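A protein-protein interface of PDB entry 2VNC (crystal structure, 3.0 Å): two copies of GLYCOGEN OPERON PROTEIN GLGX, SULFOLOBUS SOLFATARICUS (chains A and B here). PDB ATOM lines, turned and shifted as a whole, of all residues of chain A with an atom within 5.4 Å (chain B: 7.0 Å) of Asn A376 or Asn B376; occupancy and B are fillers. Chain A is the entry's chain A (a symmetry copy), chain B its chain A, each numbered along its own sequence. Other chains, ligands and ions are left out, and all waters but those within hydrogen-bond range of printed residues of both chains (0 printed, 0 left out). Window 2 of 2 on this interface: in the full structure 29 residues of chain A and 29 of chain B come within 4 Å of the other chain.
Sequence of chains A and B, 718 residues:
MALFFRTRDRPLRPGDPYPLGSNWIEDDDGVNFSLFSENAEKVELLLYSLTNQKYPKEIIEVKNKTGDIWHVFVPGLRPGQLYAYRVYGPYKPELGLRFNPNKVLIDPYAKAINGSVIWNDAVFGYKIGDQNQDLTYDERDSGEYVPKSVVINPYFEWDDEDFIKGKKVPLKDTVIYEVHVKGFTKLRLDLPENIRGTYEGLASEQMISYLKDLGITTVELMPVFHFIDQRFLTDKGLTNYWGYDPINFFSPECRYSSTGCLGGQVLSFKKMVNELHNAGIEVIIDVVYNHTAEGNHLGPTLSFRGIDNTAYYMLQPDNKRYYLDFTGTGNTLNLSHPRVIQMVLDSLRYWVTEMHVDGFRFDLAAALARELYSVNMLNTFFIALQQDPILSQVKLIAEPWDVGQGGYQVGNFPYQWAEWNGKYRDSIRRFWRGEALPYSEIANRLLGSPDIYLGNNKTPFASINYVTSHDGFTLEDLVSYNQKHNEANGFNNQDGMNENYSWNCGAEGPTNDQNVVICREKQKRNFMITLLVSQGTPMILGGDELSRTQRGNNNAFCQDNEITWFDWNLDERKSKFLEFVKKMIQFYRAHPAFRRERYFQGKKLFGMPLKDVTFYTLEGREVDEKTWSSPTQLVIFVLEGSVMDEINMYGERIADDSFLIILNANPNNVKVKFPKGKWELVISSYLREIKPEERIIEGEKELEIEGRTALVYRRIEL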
ATOM      1  N   LEU A 372      26.946   0.009  12.077  1.00  0.00           N
ATOM      2  CA  LEU A 372      28.255   0.395  11.613  1.00  0.00           C
ATOM      3  C   LEU A 372      28.142   1.112  10.280  1.00  0.00           C
ATOM      4  O   LEU A 372      28.680   2.198  10.103  1.00  0.00           O
ATOM      5  CB  LEU A 372      29.144  -0.838  11.489  1.00  0.00           C
ATOM      6  CG  LEU A 372      29.664  -1.384  12.807  1.00  0.00           C
ATOM      7  CD1 LEU A 372      30.170  -2.794  12.612  1.00  0.00           C
ATOM      8  CD2 LEU A 372      30.748  -0.484  13.313  1.00  0.00           C
ATOM      9  N   TYR A 373      27.405   0.515   9.351  1.00  0.00           N
ATOM     10  CA  TYR A 373      27.225   1.097   8.027  1.00  0.00           C
ATOM     11  C   TYR A 373      26.598   2.492   8.069  1.00  0.00           C
ATOM     12  O   TYR A 373      26.990   3.401   7.330  1.00  0.00           O
ATOM     13  CB  TYR A 373      26.367   0.172   7.202  1.00  0.00           C
ATOM     14  CG  TYR A 373      26.478   0.452   5.738  1.00  0.00           C
ATOM     15  CD1 TYR A 373      25.385   0.938   5.022  1.00  0.00           C
ATOM     16  CD2 TYR A 373      27.675   0.242   5.069  1.00  0.00           C
ATOM     17  CE1 TYR A 373      25.490   1.190   3.682  1.00  0.00           C
ATOM     18  CE2 TYR A 373      27.786   0.487   3.748  1.00  0.00           C
ATOM     19  CZ  TYR A 373      26.699   0.960   3.053  1.00  0.00           C
ATOM     20  OH  TYR A 373      26.830   1.216   1.716  1.00  0.00           O
ATOM     21  N   SER A 374      25.617   2.632   8.957  1.00  0.00           N
ATOM     22  CA  SER A 374      24.944   3.879   9.283  1.00  0.00           C
ATOM     23  C   SER A 374      25.860   5.110   9.414  1.00  0.00           C
ATOM     24  O   SER A 374      25.445   6.239   9.141  1.00  0.00           O
ATOM     25  CB  SER A 374      24.199   3.658  10.591  1.00  0.00           C
ATOM     26  OG  SER A 374      23.788   4.892  11.146  1.00  0.00           O
ATOM     27  N   VAL A 375      27.096   4.890   9.850  1.00  0.00           N
ATOM     28  CA  VAL A 375      28.041   5.979  10.093  1.00  0.00           C
ATOM     29  C   VAL A 375      29.390   5.689   9.440  1.00  0.00           C
ATOM     30  O   VAL A 375      30.418   6.246   9.828  1.00  0.00           O
ATOM     31  CB  VAL A 375      28.230   6.258  11.593  1.00  0.00           C
ATOM     32  CG1 VAL A 375      26.963   6.847  12.192  1.00  0.00           C
ATOM     33  CG2 VAL A 375      28.651   4.987  12.332  1.00  0.00           C
ATOM     34  N   ASN A 376      29.372   4.804   8.447  1.00  0.00           N
ATOM     35  CA  ASN A 376      30.531   4.572   7.578  1.00  0.00           C
ATOM     36  C   ASN A 376      31.722   3.957   8.308  1.00  0.00           C
ATOM     37  O   ASN A 376      32.865   4.360   8.130  1.00  0.00           O
ATOM     38  CB  ASN A 376      30.911   5.883   6.880  1.00  0.00           C
ATOM     39  CG  ASN A 376      31.760   5.667   5.655  1.00  0.00           C
ATOM     40  OD1 ASN A 376      32.760   6.350   5.473  1.00  0.00           O
ATOM     41  ND2 ASN A 376      31.363   4.715   4.800  1.00  0.00           N
ATOM     42  N   MET A 377      31.427   2.954   9.123  1.00  0.00           N
ATOM     43  CA  MET A 377      32.402   2.316  10.011  1.00  0.00           C
ATOM     44  C   MET A 377      32.554   0.808   9.771  1.00  0.00           C
ATOM     45  O   MET A 377      33.503   0.204  10.256  1.00  0.00           O
ATOM     46  CB  MET A 377      32.007   2.591  11.456  1.00  0.00           C
ATOM     47  CG  MET A 377      32.228   4.024  11.849  1.00  0.00           C
ATOM     48  SD  MET A 377      33.994   4.460  11.822  1.00  0.00           S
ATOM     49  CE  MET A 377      34.724   3.223  12.903  1.00  0.00           C
ATOM     50  N   LEU A 378      31.629   0.226   9.004  1.00  0.00           N
ATOM     51  CA  LEU A 378      31.626  -1.202   8.697  1.00  0.00           C
ATOM     52  C   LEU A 378      32.945  -1.705   8.114  1.00  0.00           C
ATOM     53  O   LEU A 378      33.575  -2.584   8.702  1.00  0.00           O
ATOM     54  CB  LEU A 378      30.498  -1.542   7.733  1.00  0.00           C
ATOM     55  CG  LEU A 378      29.774  -2.890   7.795  1.00  0.00           C
ATOM     56  CD1 LEU A 378      29.458  -3.345   6.380  1.00  0.00           C
ATOM     57  CD2 LEU A 378      30.486  -3.992   8.553  1.00  0.00           C
ATOM     58  N   THR A 380      35.893  -0.088   7.809  1.00  0.00           N
ATOM     59  CA  THR A 380      36.998   0.242   8.692  1.00  0.00           C
ATOM     60  C   THR A 380      36.954  -0.656   9.930  1.00  0.00           C
ATOM     61  O   THR A 380      37.981  -1.057  10.436  1.00  0.00           O
ATOM     62  CB  THR A 380      37.030   1.712   9.118  1.00  0.00           C
ATOM     63  OG1 THR A 380      36.371   1.841  10.383  1.00  0.00           O
ATOM     64  CG2 THR A 380      36.359   2.628   8.076  1.00  0.00           C
ATOM     65  N   LEU B 335      16.784   5.083   0.414  1.00  0.00           N
ATOM     66  CA  LEU B 335      17.555   5.966  -0.440  1.00  0.00           C
ATOM     67  C   LEU B 335      18.798   5.352  -1.068  1.00  0.00           C
ATOM     68  O   LEU B 335      19.469   6.018  -1.853  1.00  0.00           O
ATOM     69  CB  LEU B 335      17.999   7.191   0.365  1.00  0.00           C
ATOM     70  CG  LEU B 335      17.167   8.463   0.542  1.00  0.00           C
ATOM     71  CD1 LEU B 335      16.354   8.758  -0.696  1.00  0.00           C
ATOM     72  CD2 LEU B 335      16.270   8.364   1.730  1.00  0.00           C
ATOM     73  N   SER B 336      19.131   4.118  -0.699  1.00  0.00           N
ATOM     74  CA  SER B 336      20.278   3.413  -1.274  1.00  0.00           C
ATOM     75  C   SER B 336      19.901   2.688  -2.556  1.00  0.00           C
ATOM     76  O   SER B 336      20.737   2.473  -3.430  1.00  0.00           O
ATOM     77  CB  SER B 336      20.814   2.385  -0.279  1.00  0.00           C
ATOM     78  OG  SER B 336      19.796   1.494   0.196  1.00  0.00           O
ATOM     79  N   GLU B 371      19.647  10.270   7.088  1.00  0.00           N
ATOM     80  CA  GLU B 371      19.129   9.107   6.381  1.00  0.00           C
ATOM     81  C   GLU B 371      20.037   8.790   5.195  1.00  0.00           C
ATOM     82  O   GLU B 371      20.457   7.652   4.998  1.00  0.00           O
ATOM     83  CB  GLU B 371      17.691   9.336   5.922  1.00  0.00           C
ATOM     84  CG  GLU B 371      16.719   9.700   7.067  1.00  0.00           C
ATOM     85  CD  GLU B 371      15.276  10.054   6.610  1.00  0.00           C
ATOM     86  OE1 GLU B 371      15.000  10.156   5.387  1.00  0.00           O
ATOM     87  OE2 GLU B 371      14.413  10.231   7.504  1.00  0.00           O
ATOM     88  N   LEU B 372      20.369   9.816   4.428  1.00  0.00           N
ATOM     89  CA  LEU B 372      21.245   9.650   3.295  1.00  0.00           C
ATOM     90  C   LEU B 372      22.567   9.055   3.745  1.00  0.00           C
ATOM     91  O   LEU B 372      23.035   8.071   3.187  1.00  0.00           O
ATOM     92  CB  LEU B 372      21.464  10.995   2.609  1.00  0.00           C
ATOM     93  CG  LEU B 372      20.298  11.476   1.763  1.00  0.00           C
ATOM     94  CD1 LEU B 372      20.448  12.952   1.479  1.00  0.00           C
ATOM     95  CD2 LEU B 372      20.258  10.681   0.496  1.00  0.00           C
ATOM     96  N   TYR B 373      23.151   9.637   4.786  1.00  0.00           N
ATOM     97  CA  TYR B 373      24.426   9.165   5.310  1.00  0.00           C
ATOM     98  C   TYR B 373      24.384   7.702   5.757  1.00  0.00           C
ATOM     99  O   TYR B 373      25.317   6.928   5.527  1.00  0.00           O
ATOM    100  CB  TYR B 373      24.833  10.045   6.464  1.00  0.00           C
ATOM    101  CG  TYR B 373      26.287   9.922   6.784  1.00  0.00           C
ATOM    102  CD1 TYR B 373      26.706   9.369   7.993  1.00  0.00           C
ATOM    103  CD2 TYR B 373      27.247  10.350   5.877  1.00  0.00           C
ATOM    104  CE1 TYR B 373      28.038   9.261   8.282  1.00  0.00           C
ATOM    105  CE2 TYR B 373      28.563  10.249   6.156  1.00  0.00           C
ATOM    106  CZ  TYR B 373      28.960   9.706   7.355  1.00  0.00           C
ATOM    107  OH  TYR B 373      30.299   9.598   7.618  1.00  0.00           O
ATOM    108  N   SER B 374      23.272   7.352   6.398  1.00  0.00           N
ATOM    109  CA  SER B 374      22.927   6.003   6.816  1.00  0.00           C
ATOM    110  C   SER B 374      23.235   4.894   5.790  1.00  0.00           C
ATOM    111  O   SER B 374      23.517   3.752   6.160  1.00  0.00           O
ATOM    112  CB  SER B 374      21.439   5.999   7.138  1.00  0.00           C
ATOM    113  OG  SER B 374      20.955   4.674   7.238  1.00  0.00           O
ATOM    114  N   VAL B 375      23.157   5.231   4.508  1.00  0.00           N
ATOM    115  CA  VAL B 375      23.349   4.257   3.434  1.00  0.00           C
ATOM    116  C   VAL B 375      24.327   4.782   2.387  1.00  0.00           C
ATOM    117  O   VAL B 375      24.336   4.328   1.241  1.00  0.00           O
ATOM    118  CB  VAL B 375      22.021   3.863   2.767  1.00  0.00           C
ATOM    119  CG1 VAL B 375      21.157   3.060   3.725  1.00  0.00           C
ATOM    120  CG2 VAL B 375      21.280   5.102   2.261  1.00  0.00           C
ATOM    121  N   ASN B 376      25.146   5.747   2.795  1.00  0.00           N
ATOM    122  CA  ASN B 376      26.281   6.210   1.988  1.00  0.00           C
ATOM    123  C   ASN B 376      25.862   6.903   0.693  1.00  0.00           C
ATOM    124  O   ASN B 376      26.420   6.672  -0.372  1.00  0.00           O
ATOM    125  CB  ASN B 376      27.225   5.033   1.718  1.00  0.00           C
ATOM    126  CG  ASN B 376      28.607   5.473   1.313  1.00  0.00           C
ATOM    127  OD1 ASN B 376      29.164   4.947   0.357  1.00  0.00           O
ATOM    128  ND2 ASN B 376      29.174   6.442   2.043  1.00  0.00           N
ATOM    129  N   MET B 377      24.873   7.777   0.818  1.00  0.00           N
ATOM    130  CA  MET B 377      24.235   8.448  -0.318  1.00  0.00           C
ATOM    131  C   MET B 377      24.312   9.979  -0.244  1.00  0.00           C
ATOM    132  O   MET B 377      24.053  10.653  -1.235  1.00  0.00           O
ATOM    133  CB  MET B 377      22.788   7.988  -0.417  1.00  0.00           C
ATOM    134  CG  MET B 377      22.668   6.565  -0.884  1.00  0.00           C
ATOM    135  SD  MET B 377      23.272   6.368  -2.588  1.00  0.00           S
ATOM    136  CE  MET B 377      22.303   7.581  -3.495  1.00  0.00           C
ATOM    137  N   LEU B 378      24.688  10.506   0.922  1.00  0.00           N
ATOM    138  CA  LEU B 378      24.791  11.944   1.157  1.00  0.00           C
ATOM    139  C   LEU B 378      25.667  12.669   0.135  1.00  0.00           C
ATOM    140  O   LEU B 378      25.183  13.562  -0.558  1.00  0.00           O
ATOM    141  CB  LEU B 378      25.327  12.225   2.553  1.00  0.00           C
ATOM    142  CG  LEU B 378      24.878  13.455   3.348  1.00  0.00           C
ATOM    143  CD1 LEU B 378      26.064  13.998   4.127  1.00  0.00           C
ATOM    144  CD2 LEU B 378      24.227  14.563   2.546  1.00  0.00           C
ATOM    145  N   ASN B 379      26.944  12.300   0.025  1.00  0.00           N
ATOM    146  CA  ASN B 379      27.807  12.983  -0.938  1.00  0.00           C
ATOM    147  C   ASN B 379      27.446  12.709  -2.402  1.00  0.00           C
ATOM    148  O   ASN B 379      27.516  13.616  -3.238  1.00  0.00           O
ATOM    149  CB  ASN B 379      29.297  12.759  -0.675  1.00  0.00           C
ATOM    150  CG  ASN B 379      30.183  13.741  -1.475  1.00  0.00           C
ATOM    151  OD1 ASN B 379      30.019  14.980  -1.399  1.00  0.00           O
ATOM    152  ND2 ASN B 379      31.118  13.184  -2.254  1.00  0.00           N
ATOM    153  N   THR B 380      27.037  11.486  -2.714  1.00  0.00           N
ATOM    154  CA  THR B 380      26.571  11.221  -4.065  1.00  0.00           C
ATOM    155  C   THR B 380      25.269  11.983  -4.319  1.00  0.00           C
ATOM    156  O   THR B 380      25.041  12.465  -5.409  1.00  0.00           O
ATOM    157  CB  THR B 380      26.369   9.733  -4.365  1.00  0.00           C
ATOM    158  OG1 THR B 380      24.994   9.400  -4.144  1.00  0.00           O
ATOM    159  CG2 THR B 380      27.277   8.842  -3.497  1.00  0.00           C
ATOM    160  N   PHE B 381      24.417  12.118  -3.315  1.00  0.00           N
ATOM    161  CA  PHE B 381      23.195  12.885  -3.508  1.00  0.00           C
ATOM    162  C   PHE B 381      23.524  14.313  -3.839  1.00  0.00           C
ATOM    163  O   PHE B 381      22.802  14.949  -4.593  1.00  0.00           O
ATOM    164  CB  PHE B 381      22.281  12.840  -2.284  1.00  0.00           C
ATOM    165  CG  PHE B 381      21.048  13.726  -2.400  1.00  0.00           C
ATOM    166  CD1 PHE B 381      20.929  14.889  -1.628  1.00  0.00           C
ATOM    167  CD2 PHE B 381      20.001  13.388  -3.270  1.00  0.00           C
ATOM    168  CE1 PHE B 381      19.800  15.692  -1.721  1.00  0.00           C
ATOM    169  CE2 PHE B 381      18.872  14.192  -3.360  1.00  0.00           C
ATOM    170  CZ  PHE B 381      18.778  15.344  -2.584  1.00  0.00           C
ATOM    171  N   GLN B 409      30.180  16.882   6.030  1.00  0.00           N
ATOM    172  CA  GLN B 409      30.621  15.570   5.572  1.00  0.00           C
ATOM    173  C   GLN B 409      30.582  15.475   4.051  1.00  0.00           C
ATOM    174  O   GLN B 409      30.360  14.401   3.493  1.00  0.00           O
ATOM    175  CB  GLN B 409      29.758  14.469   6.191  1.00  0.00           C
ATOM    176  CG  GLN B 409      30.377  13.805   7.410  1.00  0.00           C
ATOM    177  CD  GLN B 409      31.888  13.721   7.323  1.00  0.00           C
ATOM    178  OE1 GLN B 409      32.603  14.386   8.073  1.00  0.00           O
ATOM    179  NE2 GLN B 409      32.383  12.900   6.404  1.00  0.00           N
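Among the printed residues, merely in contact across the chains: Ser A374 with Ser B374, Tyr A373 with Ser B374, Ser A374 with Tyr B373, Val A375 with Tyr B373, Tyr A373 with Val B375, Asn A376 with Tyr B373, Tyr A373 with Asn B376 and Asn A376 with Asn B376.
Of the 14 printed residues of chain B, 4 touch a printed residue of chain A. Of the 8 printed residues of chain A, 4 touch a printed residue of chain B. Printed residues of chain A that touch a printed residue of chain B: Tyr A373, Ser A374, Val A375 and Asn A376. Hydrophobic or aromatic side chains of chain A within 4 Å of the printed part of chain B: Tyr A373. Among the printed residues, 8 pairs touch across the chains. Among the printed residues, no Asp or Glu carboxylate lies within 4 Å of a Lys or Arg side-chain nitrogen of the other chain.
Tyr A373 touches Val B375, and with the chains exchanged Val A375 touches Tyr B373. Tyr A373 touches Asn B376, and with the chains exchanged Asn A376 touches Tyr B373. Ser B374 touches its own counterpart, Ser A374. Asn A376 touches its own counterpart, Asn B376. 8 positions are printed for both chains.
Of chain B, only Tyr B373 (3.8 Å) and Asn B376 (3.9 Å) come within 4 Å of Asn A376. Asn B376 touches just these residues of chain A: Tyr A373 (3.8 Å) and Asn A376 (3.9 Å). Of the printed residues of chain A, Val B375 touches Tyr A373. Printed residues of chain B within 4 Å of Tyr A373: Ser B374, Val B375 and Asn B376. Of the printed residues of chain A, Ser B374 touches Tyr A373 (3.6 Å) and Ser A374 (3.4 Å). Printed residues of chain B within 4 Å of Ser A374: Tyr B373 and Ser B374. Glu B371 touches none of the printed residues of chain A. The nearest printed residue of chain A that does not touch Asn B376 is Ser A374 (6.4 Å). The nearest printed residue of chain A that does not touch Ser B374 is Val A375 (5.3 Å).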
